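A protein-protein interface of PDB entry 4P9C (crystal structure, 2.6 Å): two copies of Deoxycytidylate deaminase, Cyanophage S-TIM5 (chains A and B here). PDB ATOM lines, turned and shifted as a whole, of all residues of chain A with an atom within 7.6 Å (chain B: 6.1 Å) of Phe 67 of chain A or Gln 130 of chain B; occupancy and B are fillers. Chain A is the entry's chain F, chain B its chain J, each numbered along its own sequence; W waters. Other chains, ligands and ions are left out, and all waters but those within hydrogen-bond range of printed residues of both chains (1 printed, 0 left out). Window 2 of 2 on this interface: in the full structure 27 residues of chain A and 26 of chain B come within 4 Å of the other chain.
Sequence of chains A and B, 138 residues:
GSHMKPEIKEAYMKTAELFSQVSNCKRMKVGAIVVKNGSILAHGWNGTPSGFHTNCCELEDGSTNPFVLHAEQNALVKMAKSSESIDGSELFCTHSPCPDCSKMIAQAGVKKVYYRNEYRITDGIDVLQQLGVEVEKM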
ATOM      1  N   GLY A  47      12.685  16.927  -3.034  1.00  0.00           N
ATOM      2  CA  GLY A  47      13.659  16.069  -3.689  1.00  0.00           C
ATOM      3  C   GLY A  47      13.272  15.767  -5.121  1.00  0.00           C
ATOM      4  O   GLY A  47      12.172  16.111  -5.567  1.00  0.00           O
ATOM      5  N   THR A  48      14.187  15.127  -5.842  1.00  0.00           N
ATOM      6  CA  THR A  48      13.956  14.718  -7.222  1.00  0.00           C
ATOM      7  C   THR A  48      12.954  13.560  -7.256  1.00  0.00           C
ATOM      8  O   THR A  48      12.778  12.876  -6.249  1.00  0.00           O
ATOM      9  CB  THR A  48      15.277  14.301  -7.914  1.00  0.00           C
ATOM     10  OG1 THR A  48      15.954  13.322  -7.120  1.00  0.00           O
ATOM     11  CG2 THR A  48      16.189  15.506  -8.120  1.00  0.00           C
ATOM     12  N   PRO A  49      12.290  13.337  -8.410  1.00  0.00           N
ATOM     13  CA  PRO A  49      11.325  12.236  -8.495  1.00  0.00           C
ATOM     14  C   PRO A  49      11.982  10.875  -8.272  1.00  0.00           C
ATOM     15  O   PRO A  49      13.205  10.752  -8.381  1.00  0.00           O
ATOM     16  CB  PRO A  49      10.792  12.333  -9.929  1.00  0.00           C
ATOM     17  CG  PRO A  49      11.152  13.696 -10.398  1.00  0.00           C
ATOM     18  CD  PRO A  49      12.421  14.041  -9.698  1.00  0.00           C
ATOM     19  N   SER A  50      11.172   9.869  -7.951  1.00  0.00           N
ATOM     20  CA  SER A  50      11.668   8.514  -7.733  1.00  0.00           C
ATOM     21  C   SER A  50      12.348   7.981  -8.987  1.00  0.00           C
ATOM     22  O   SER A  50      11.762   7.975 -10.075  1.00  0.00           O
ATOM     23  CB  SER A  50      10.529   7.579  -7.319  1.00  0.00           C
ATOM     24  OG  SER A  50       9.947   7.989  -6.086  1.00  0.00           O
ATOM     25  N   GLY A  51      13.598   7.554  -8.825  1.00  0.00           N
ATOM     26  CA  GLY A  51      14.363   6.919  -9.899  1.00  0.00           C
ATOM     27  C   GLY A  51      14.955   7.874 -10.920  1.00  0.00           C
ATOM     28  O   GLY A  51      15.362   7.456 -12.008  1.00  0.00           O
ATOM     29  N   PHE A  52      14.999   9.157 -10.567  1.00  0.00           N
ATOM     30  CA  PHE A  52      15.585  10.192 -11.411  1.00  0.00           C
ATOM     31  C   PHE A  52      17.101   9.976 -11.456  1.00  0.00           C
ATOM     32  O   PHE A  52      17.675   9.445 -10.502  1.00  0.00           O
ATOM     33  CB  PHE A  52      15.229  11.563 -10.831  1.00  0.00           C
ATOM     34  CG  PHE A  52      15.468  12.713 -11.765  1.00  0.00           C
ATOM     35  CD1 PHE A  52      14.705  12.868 -12.919  1.00  0.00           C
ATOM     36  CD2 PHE A  52      16.440  13.663 -11.471  1.00  0.00           C
ATOM     37  CE1 PHE A  52      14.926  13.944 -13.778  1.00  0.00           C
ATOM     38  CE2 PHE A  52      16.669  14.741 -12.320  1.00  0.00           C
ATOM     39  CZ  PHE A  52      15.911  14.881 -13.476  1.00  0.00           C
ATOM     40  N   HIS A  53      17.743  10.381 -12.551  1.00  0.00           N
ATOM     41  CA  HIS A  53      19.172  10.102 -12.767  1.00  0.00           C
ATOM     42  C   HIS A  53      20.091  10.611 -11.649  1.00  0.00           C
ATOM     43  O   HIS A  53      21.190  10.084 -11.459  1.00  0.00           O
ATOM     44  CB  HIS A  53      19.638  10.641 -14.122  1.00  0.00           C
ATOM     45  CG  HIS A  53      19.740  12.133 -14.183  1.00  0.00           C
ATOM     46  ND1 HIS A  53      20.890  12.816 -13.850  1.00  0.00           N
ATOM     47  CD2 HIS A  53      18.836  13.074 -14.545  1.00  0.00           C
ATOM     48  CE1 HIS A  53      20.691  14.113 -14.004  1.00  0.00           C
ATOM     49  NE2 HIS A  53      19.451  14.296 -14.424  1.00  0.00           N
ATOM     50  N   CYS A  56      20.603  15.218  -6.659  1.00  0.00           N
ATOM     51  CA  CYS A  56      20.879  16.601  -6.504  1.00  0.00           C
ATOM     52  C   CYS A  56      19.698  17.386  -6.823  1.00  0.00           C
ATOM     53  O   CYS A  56      19.134  17.210  -7.836  1.00  0.00           O
ATOM     54  CB  CYS A  56      21.994  16.995  -7.448  1.00  0.00           C
ATOM     55  SG  CYS A  56      22.922  18.368  -6.970  1.00  0.00           S
ATOM     56  N   CYS A  57      19.304  18.257  -5.900  1.00  0.00           N
ATOM     57  CA  CYS A  57      18.097  19.048  -6.055  1.00  0.00           C
ATOM     58  C   CYS A  57      18.373  20.367  -6.757  1.00  0.00           C
ATOM     59  O   CYS A  57      17.442  21.092  -7.106  1.00  0.00           O
ATOM     60  CB  CYS A  57      17.450  19.311  -4.689  1.00  0.00           C
ATOM     61  SG  CYS A  57      17.047  17.816  -3.756  1.00  0.00           S
ATOM     62  N   LEU A  59      20.589  22.576  -9.867  1.00  0.00           N
ATOM     63  CA  LEU A  59      21.312  22.468 -11.129  1.00  0.00           C
ATOM     64  C   LEU A  59      22.751  22.953 -10.981  1.00  0.00           C
ATOM     65  O   LEU A  59      23.296  22.980  -9.879  1.00  0.00           O
ATOM     66  CB  LEU A  59      20.599  23.260 -12.225  1.00  0.00           C
ATOM     67  CG  LEU A  59      20.123  22.461 -13.439  1.00  0.00           C
ATOM     68  CD1 LEU A  59      19.115  21.401 -13.024  1.00  0.00           C
ATOM     69  CD2 LEU A  59      19.533  23.384 -14.495  1.00  0.00           C
ATOM     70  N   THR A  64      17.287  25.549  -8.259  1.00  0.00           N
ATOM     71  CA  THR A  64      16.660  24.237  -8.088  1.00  0.00           C
ATOM     72  C   THR A  64      16.213  23.658  -9.435  1.00  0.00           C
ATOM     73  O   THR A  64      15.594  24.356 -10.243  1.00  0.00           O
ATOM     74  CB  THR A  64      15.455  24.310  -7.115  1.00  0.00           C
ATOM     75  OG1 THR A  64      15.885  24.845  -5.856  1.00  0.00           O
ATOM     76  CG2 THR A  64      14.848  22.931  -6.879  1.00  0.00           C
ATOM     77  N   ASN A  65      16.555  22.392  -9.670  1.00  0.00           N
ATOM     78  CA  ASN A  65      16.059  21.626 -10.814  1.00  0.00           C
ATOM     79  C   ASN A  65      14.532  21.695 -10.864  1.00  0.00           C
ATOM     80  O   ASN A  65      13.872  21.447  -9.853  1.00  0.00           O
ATOM     81  CB  ASN A  65      16.518  20.161 -10.702  1.00  0.00           C
ATOM     82  CG  ASN A  65      16.465  19.404 -12.028  1.00  0.00           C
ATOM     83  OD1 ASN A  65      15.585  19.625 -12.860  1.00  0.00           O
ATOM     84  ND2 ASN A  65      17.406  18.488 -12.217  1.00  0.00           N
ATOM     85  N   PRO A  66      13.964  22.058 -12.032  1.00  0.00           N
ATOM     86  CA  PRO A  66      12.506  22.056 -12.207  1.00  0.00           C
ATOM     87  C   PRO A  66      11.844  20.685 -12.002  1.00  0.00           C
ATOM     88  O   PRO A  66      10.629  20.621 -11.823  1.00  0.00           O
ATOM     89  CB  PRO A  66      12.316  22.541 -13.655  1.00  0.00           C
ATOM     90  CG  PRO A  66      13.680  22.513 -14.284  1.00  0.00           C
ATOM     91  CD  PRO A  66      14.651  22.700 -13.169  1.00  0.00           C
ATOM     92  N   PHE A  67      12.635  19.612 -12.023  1.00  0.00           N
ATOM     93  CA  PHE A  67      12.130  18.251 -11.792  1.00  0.00           C
ATOM     94  C   PHE A  67      11.836  17.961 -10.315  1.00  0.00           C
ATOM     95  O   PHE A  67      11.057  17.060  -9.995  1.00  0.00           O
ATOM     96  CB  PHE A  67      13.105  17.202 -12.356  1.00  0.00           C
ATOM     97  CG  PHE A  67      12.986  17.000 -13.849  1.00  0.00           C
ATOM     98  CD1 PHE A  67      12.096  16.062 -14.370  1.00  0.00           C
ATOM     99  CD2 PHE A  67      13.762  17.744 -14.732  1.00  0.00           C
ATOM    100  CE1 PHE A  67      11.985  15.869 -15.750  1.00  0.00           C
ATOM    101  CE2 PHE A  67      13.659  17.561 -16.114  1.00  0.00           C
ATOM    102  CZ  PHE A  67      12.767  16.622 -16.622  1.00  0.00           C
ATOM    103  N   VAL A  68      12.455  18.741  -9.433  1.00  0.00           N
ATOM    104  CA  VAL A  68      12.329  18.570  -7.985  1.00  0.00           C
ATOM    105  C   VAL A  68      10.913  18.867  -7.500  1.00  0.00           C
ATOM    106  O   VAL A  68      10.345  19.918  -7.809  1.00  0.00           O
ATOM    107  CB  VAL A  68      13.346  19.464  -7.226  1.00  0.00           C
ATOM    108  CG1 VAL A  68      13.074  19.475  -5.718  1.00  0.00           C
ATOM    109  CG2 VAL A  68      14.762  18.992  -7.509  1.00  0.00           C
ATOM    110  N   LEU A  69      10.353  17.923  -6.748  1.00  0.00           N
ATOM    111  CA  LEU A  69       9.040  18.091  -6.136  1.00  0.00           C
ATOM    112  C   LEU A  69       9.178  18.765  -4.779  1.00  0.00           C
ATOM    113  O   LEU A  69      10.067  18.425  -3.999  1.00  0.00           O
ATOM    114  CB  LEU A  69       8.331  16.743  -5.969  1.00  0.00           C
ATOM    115  CG  LEU A  69       7.927  15.967  -7.222  1.00  0.00           C
ATOM    116  CD1 LEU A  69       8.987  14.940  -7.579  1.00  0.00           C
ATOM    117  CD2 LEU A  69       6.585  15.288  -7.010  1.00  0.00           C
ATOM    118  N   HIS A  70       8.295  19.723  -4.509  1.00  0.00           N
ATOM    119  CA  HIS A  70       8.225  20.386  -3.207  1.00  0.00           C
ATOM    120  C   HIS A  70       7.717  19.416  -2.145  1.00  0.00           C
ATOM    121  O   HIS A  70       7.043  18.429  -2.468  1.00  0.00           O
ATOM    122  CB  HIS A  70       7.301  21.610  -3.278  1.00  0.00           C
ATOM    123  CG  HIS A  70       7.878  22.773  -4.029  1.00  0.00           C
ATOM    124  ND1 HIS A  70       7.343  24.041  -3.958  1.00  0.00           N
ATOM    125  CD2 HIS A  70       8.939  22.860  -4.867  1.00  0.00           C
ATOM    126  CE1 HIS A  70       8.051  24.859  -4.716  1.00  0.00           C
ATOM    127  NE2 HIS A  70       9.025  24.166  -5.281  1.00  0.00           N
ATOM    128  N   GLN A  73       3.995  19.111  -2.434  1.00  0.00           N
ATOM    129  CA  GLN A  73       3.618  18.292  -3.592  1.00  0.00           C
ATOM    130  C   GLN A  73       3.714  16.807  -3.267  1.00  0.00           C
ATOM    131  O   GLN A  73       2.769  16.055  -3.499  1.00  0.00           O
ATOM    132  CB  GLN A  73       4.519  18.590  -4.795  1.00  0.00           C
ATOM    133  CG  GLN A  73       4.122  19.794  -5.633  1.00  0.00           C
ATOM    134  CD  GLN A  73       5.048  19.992  -6.829  1.00  0.00           C
ATOM    135  OE1 GLN A  73       6.268  20.071  -6.678  1.00  0.00           O
ATOM    136  NE2 GLN A  73       4.468  20.076  -8.019  1.00  0.00           N
ATOM    137  N   LYS B 103       5.165  15.915 -13.868  1.00  0.00           N
ATOM    138  CA  LYS B 103       6.056  15.698 -12.739  1.00  0.00           C
ATOM    139  C   LYS B 103       5.318  14.928 -11.642  1.00  0.00           C
ATOM    140  O   LYS B 103       5.834  13.940 -11.114  1.00  0.00           O
ATOM    141  CB  LYS B 103       6.538  17.050 -12.207  1.00  0.00           C
ATOM    142  CG  LYS B 103       7.729  17.002 -11.259  1.00  0.00           C
ATOM    143  CD  LYS B 103       7.713  18.182 -10.281  1.00  0.00           C
ATOM    144  CE  LYS B 103       7.837  19.533 -10.985  1.00  0.00           C
ATOM    145  NZ  LYS B 103       7.801  20.664 -10.014  1.00  0.00           N
ATOM    146  N   ILE B 125       5.155  15.364 -22.517  1.00  0.00           N
ATOM    147  CA  ILE B 125       5.333  13.995 -23.008  1.00  0.00           C
ATOM    148  C   ILE B 125       6.754  13.511 -22.703  1.00  0.00           C
ATOM    149  O   ILE B 125       6.944  12.395 -22.218  1.00  0.00           O
ATOM    150  CB  ILE B 125       5.042  13.894 -24.532  1.00  0.00           C
ATOM    151  CG1 ILE B 125       3.593  14.298 -24.829  1.00  0.00           C
ATOM    152  CG2 ILE B 125       5.321  12.481 -25.056  1.00  0.00           C
ATOM    153  CD1 ILE B 125       3.333  14.691 -26.284  1.00  0.00           C
ATOM    154  N   ASP B 126       7.735  14.368 -22.982  1.00  0.00           N
ATOM    155  CA  ASP B 126       9.137  14.076 -22.687  1.00  0.00           C
ATOM    156  C   ASP B 126       9.367  13.835 -21.189  1.00  0.00           C
ATOM    157  O   ASP B 126      10.093  12.914 -20.821  1.00  0.00           O
ATOM    158  CB  ASP B 126      10.056  15.195 -23.202  1.00  0.00           C
ATOM    159  CG  ASP B 126       9.993  15.371 -24.721  1.00  0.00           C
ATOM    160  OD1 ASP B 126       9.638  14.408 -25.438  1.00  0.00           O
ATOM    161  OD2 ASP B 126      10.310  16.482 -25.196  1.00  0.00           O
ATOM    162  N   VAL B 127       8.737  14.654 -20.344  1.00  0.00           N
ATOM    163  CA  VAL B 127       8.844  14.517 -18.882  1.00  0.00           C
ATOM    164  C   VAL B 127       8.264  13.179 -18.407  1.00  0.00           C
ATOM    165  O   VAL B 127       8.898  12.462 -17.625  1.00  0.00           O
ATOM    166  CB  VAL B 127       8.165  15.709 -18.145  1.00  0.00           C
ATOM    167  CG1 VAL B 127       8.119  15.475 -16.637  1.00  0.00           C
ATOM    168  CG2 VAL B 127       8.891  17.012 -18.454  1.00  0.00           C
ATOM    169  N   LEU B 128       7.064  12.861 -18.890  1.00  0.00           N
ATOM    170  CA  LEU B 128       6.416  11.571 -18.636  1.00  0.00           C
ATOM    171  C   LEU B 128       7.275  10.378 -19.071  1.00  0.00           C
ATOM    172  O   LEU B 128       7.438   9.420 -18.313  1.00  0.00           O
ATOM    173  CB  LEU B 128       5.055  11.525 -19.343  1.00  0.00           C
ATOM    174  CG  LEU B 128       3.725  11.465 -18.573  1.00  0.00           C
ATOM    175  CD1 LEU B 128       3.789  12.038 -17.156  1.00  0.00           C
ATOM    176  CD2 LEU B 128       2.599  12.113 -19.380  1.00  0.00           C
ATOM    177  N   GLN B 129       7.822  10.446 -20.283  1.00  0.00           N
ATOM    178  CA  GLN B 129       8.628   9.352 -20.829  1.00  0.00           C
ATOM    179  C   GLN B 129       9.981   9.200 -20.131  1.00  0.00           C
ATOM    180  O   GLN B 129      10.476   8.080 -19.973  1.00  0.00           O
ATOM    181  CB  GLN B 129       8.807   9.507 -22.341  1.00  0.00           C
ATOM    182  CG  GLN B 129       7.528   9.263 -23.130  1.00  0.00           C
ATOM    183  CD  GLN B 129       7.715   9.390 -24.629  1.00  0.00           C
ATOM    184  OE1 GLN B 129       8.412  10.286 -25.110  1.00  0.00           O
ATOM    185  NE2 GLN B 129       7.083   8.496 -25.378  1.00  0.00           N
ATOM    186  N   GLN B 130      10.568  10.325 -19.715  1.00  0.00           N
ATOM    187  CA  GLN B 130      11.841  10.335 -18.978  1.00  0.00           C
ATOM    188  C   GLN B 130      11.699   9.793 -17.560  1.00  0.00           C
ATOM    189  O   GLN B 130      12.686   9.389 -16.937  1.00  0.00           O
ATOM    190  CB  GLN B 130      12.430  11.749 -18.922  1.00  0.00           C
ATOM    191  CG  GLN B 130      13.138  12.194 -20.194  1.00  0.00           C
ATOM    192  CD  GLN B 130      13.521  13.666 -20.178  1.00  0.00           C
ATOM    193  OE1 GLN B 130      13.967  14.196 -19.159  1.00  0.00           O
ATOM    194  NE2 GLN B 130      13.354  14.330 -21.313  1.00  0.00           N
ATOM    195  N   LEU B 131      10.464   9.787 -17.057  1.00  0.00           N
ATOM    196  CA  LEU B 131      10.183   9.324 -15.702  1.00  0.00           C
ATOM    197  C   LEU B 131       9.539   7.938 -15.647  1.00  0.00           C
ATOM    198  O   LEU B 131       9.179   7.455 -14.566  1.00  0.00           O
ATOM    199  CB  LEU B 131       9.351  10.363 -14.942  1.00  0.00           C
ATOM    200  CG  LEU B 131      10.104  11.644 -14.564  1.00  0.00           C
ATOM    201  CD1 LEU B 131       9.143  12.747 -14.139  1.00  0.00           C
ATOM    202  CD2 LEU B 131      11.151  11.392 -13.481  1.00  0.00           C
ATOM    203  N   GLY B 132       9.414   7.300 -16.808  1.00  0.00           N
ATOM    204  CA  GLY B 132       8.971   5.907 -16.886  1.00  0.00           C
ATOM    205  C   GLY B 132       7.468   5.740 -16.968  1.00  0.00           C
ATOM    206  O   GLY B 132       6.913   4.776 -16.434  1.00  0.00           O
ATOM    207  N   VAL B 133       6.813   6.686 -17.637  1.00  0.00           N
ATOM    208  CA  VAL B 133       5.368   6.636 -17.832  1.00  0.00           C
ATOM    209  C   VAL B 133       5.092   6.428 -19.311  1.00  0.00           C
ATOM    210  O   VAL B 133       5.602   7.167 -20.161  1.00  0.00           O
ATOM    211  CB  VAL B 133       4.668   7.921 -17.325  1.00  0.00           C
ATOM    212  CG1 VAL B 133       3.166   7.863 -17.576  1.00  0.00           C
ATOM    213  CG2 VAL B 133       4.944   8.130 -15.847  1.00  0.00           C
HETATM  214  O   HOH W   1       6.686  22.817  -8.540  1.00  0.00           O
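O of Gly 47 of chain A lies within hydrogen-bond range of N of Leu 69 of chain A, at 2.8 Å.
OD1 of Asn 65 of chain A lies close to N of Phe 67 of chain A (3.1 Å).
OE1 of Gln 73 of chain A lies within hydrogen-bond range of N of His 70 of chain A, at 3.0 Å.
CD2 of Leu 131 of chain B touches CB of Pro 49 of chain A, at 3.7 Å.
Phe 52 of chain A touches Leu 131 of chain B.
Phe 67 of chain A touches Lys 103 of chain B (O to CD, 3.5 Å).
Phe 67 of chain A touches Val 127 of chain B (CE1 to CG1, 3.99 Å).
Phe 67 of chain A touches Gln 130 of chain B.
Lys 103 of chain B touches Leu 69 of chain A.
OE1 of Gln 73 of chain A touches NZ of Lys 103 of chain B, 3.7 Å away.
Water W1 bridges NZ of Lys 103 of chain B (2.8 Å) and OE1 of Gln 73 of chain A (3.3 Å).
Of the 18 printed residues of chain A, 7 touch a printed residue of chain B.
Hydrophobic or aromatic side chains of chain A that line the printed part of chain B: Pro 49, Phe 52, Phe 67 and Leu 69.
Of the 10 printed residues of chain B, 4 touch a printed residue of chain A.
Printed residues of chain B that touch a printed residue of chain A: Lys 103, Val 127, Gln 130 and Leu 131.
Among the printed residues, no Asp or Glu carboxylate lies within 4 Å of a Lys or Arg side-chain nitrogen of the other chain.
Printed residues of chain B within 4 Å of Phe 67 of chain A: Lys 103 (3.5 Å), Val 127 (3.99 Å) and Gln 130 (3.7 Å).
Gln 130 of chain B touches just one residue of chain A: Phe 67 (3.7 Å).
Printed residues of chain B within 4 Å of Pro 66 of chain A: Lys 103.
Printed residues of chain B within 4 Å of Gln 73 of chain A: Lys 103.
Thr 64 of chain A touches none of the printed residues of chain B.
Cys 56 of chain A touches none of the printed residues of chain B.
The nearest printed residue of chain B that does not touch Phe 67 of chain A is Leu 131 of chain B (4.4 Å).
The nearest residue of chain A that does not touch Gln 130 of chain B is Phe 52 of chain A (5.5 Å).
The nearest printed residue of chain B that does not touch Gln 73 of chain A is Val 127 of chain B (10.4 Å).
O of Pro 66 of chain A lies close to NZ of Lys 103 of chain B (3.4 Å).
O of Val 68 of chain A is in hydrogen-bond range of NZ of Lys 103 of chain B (3.4 Å).
No position is printed for both chains.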
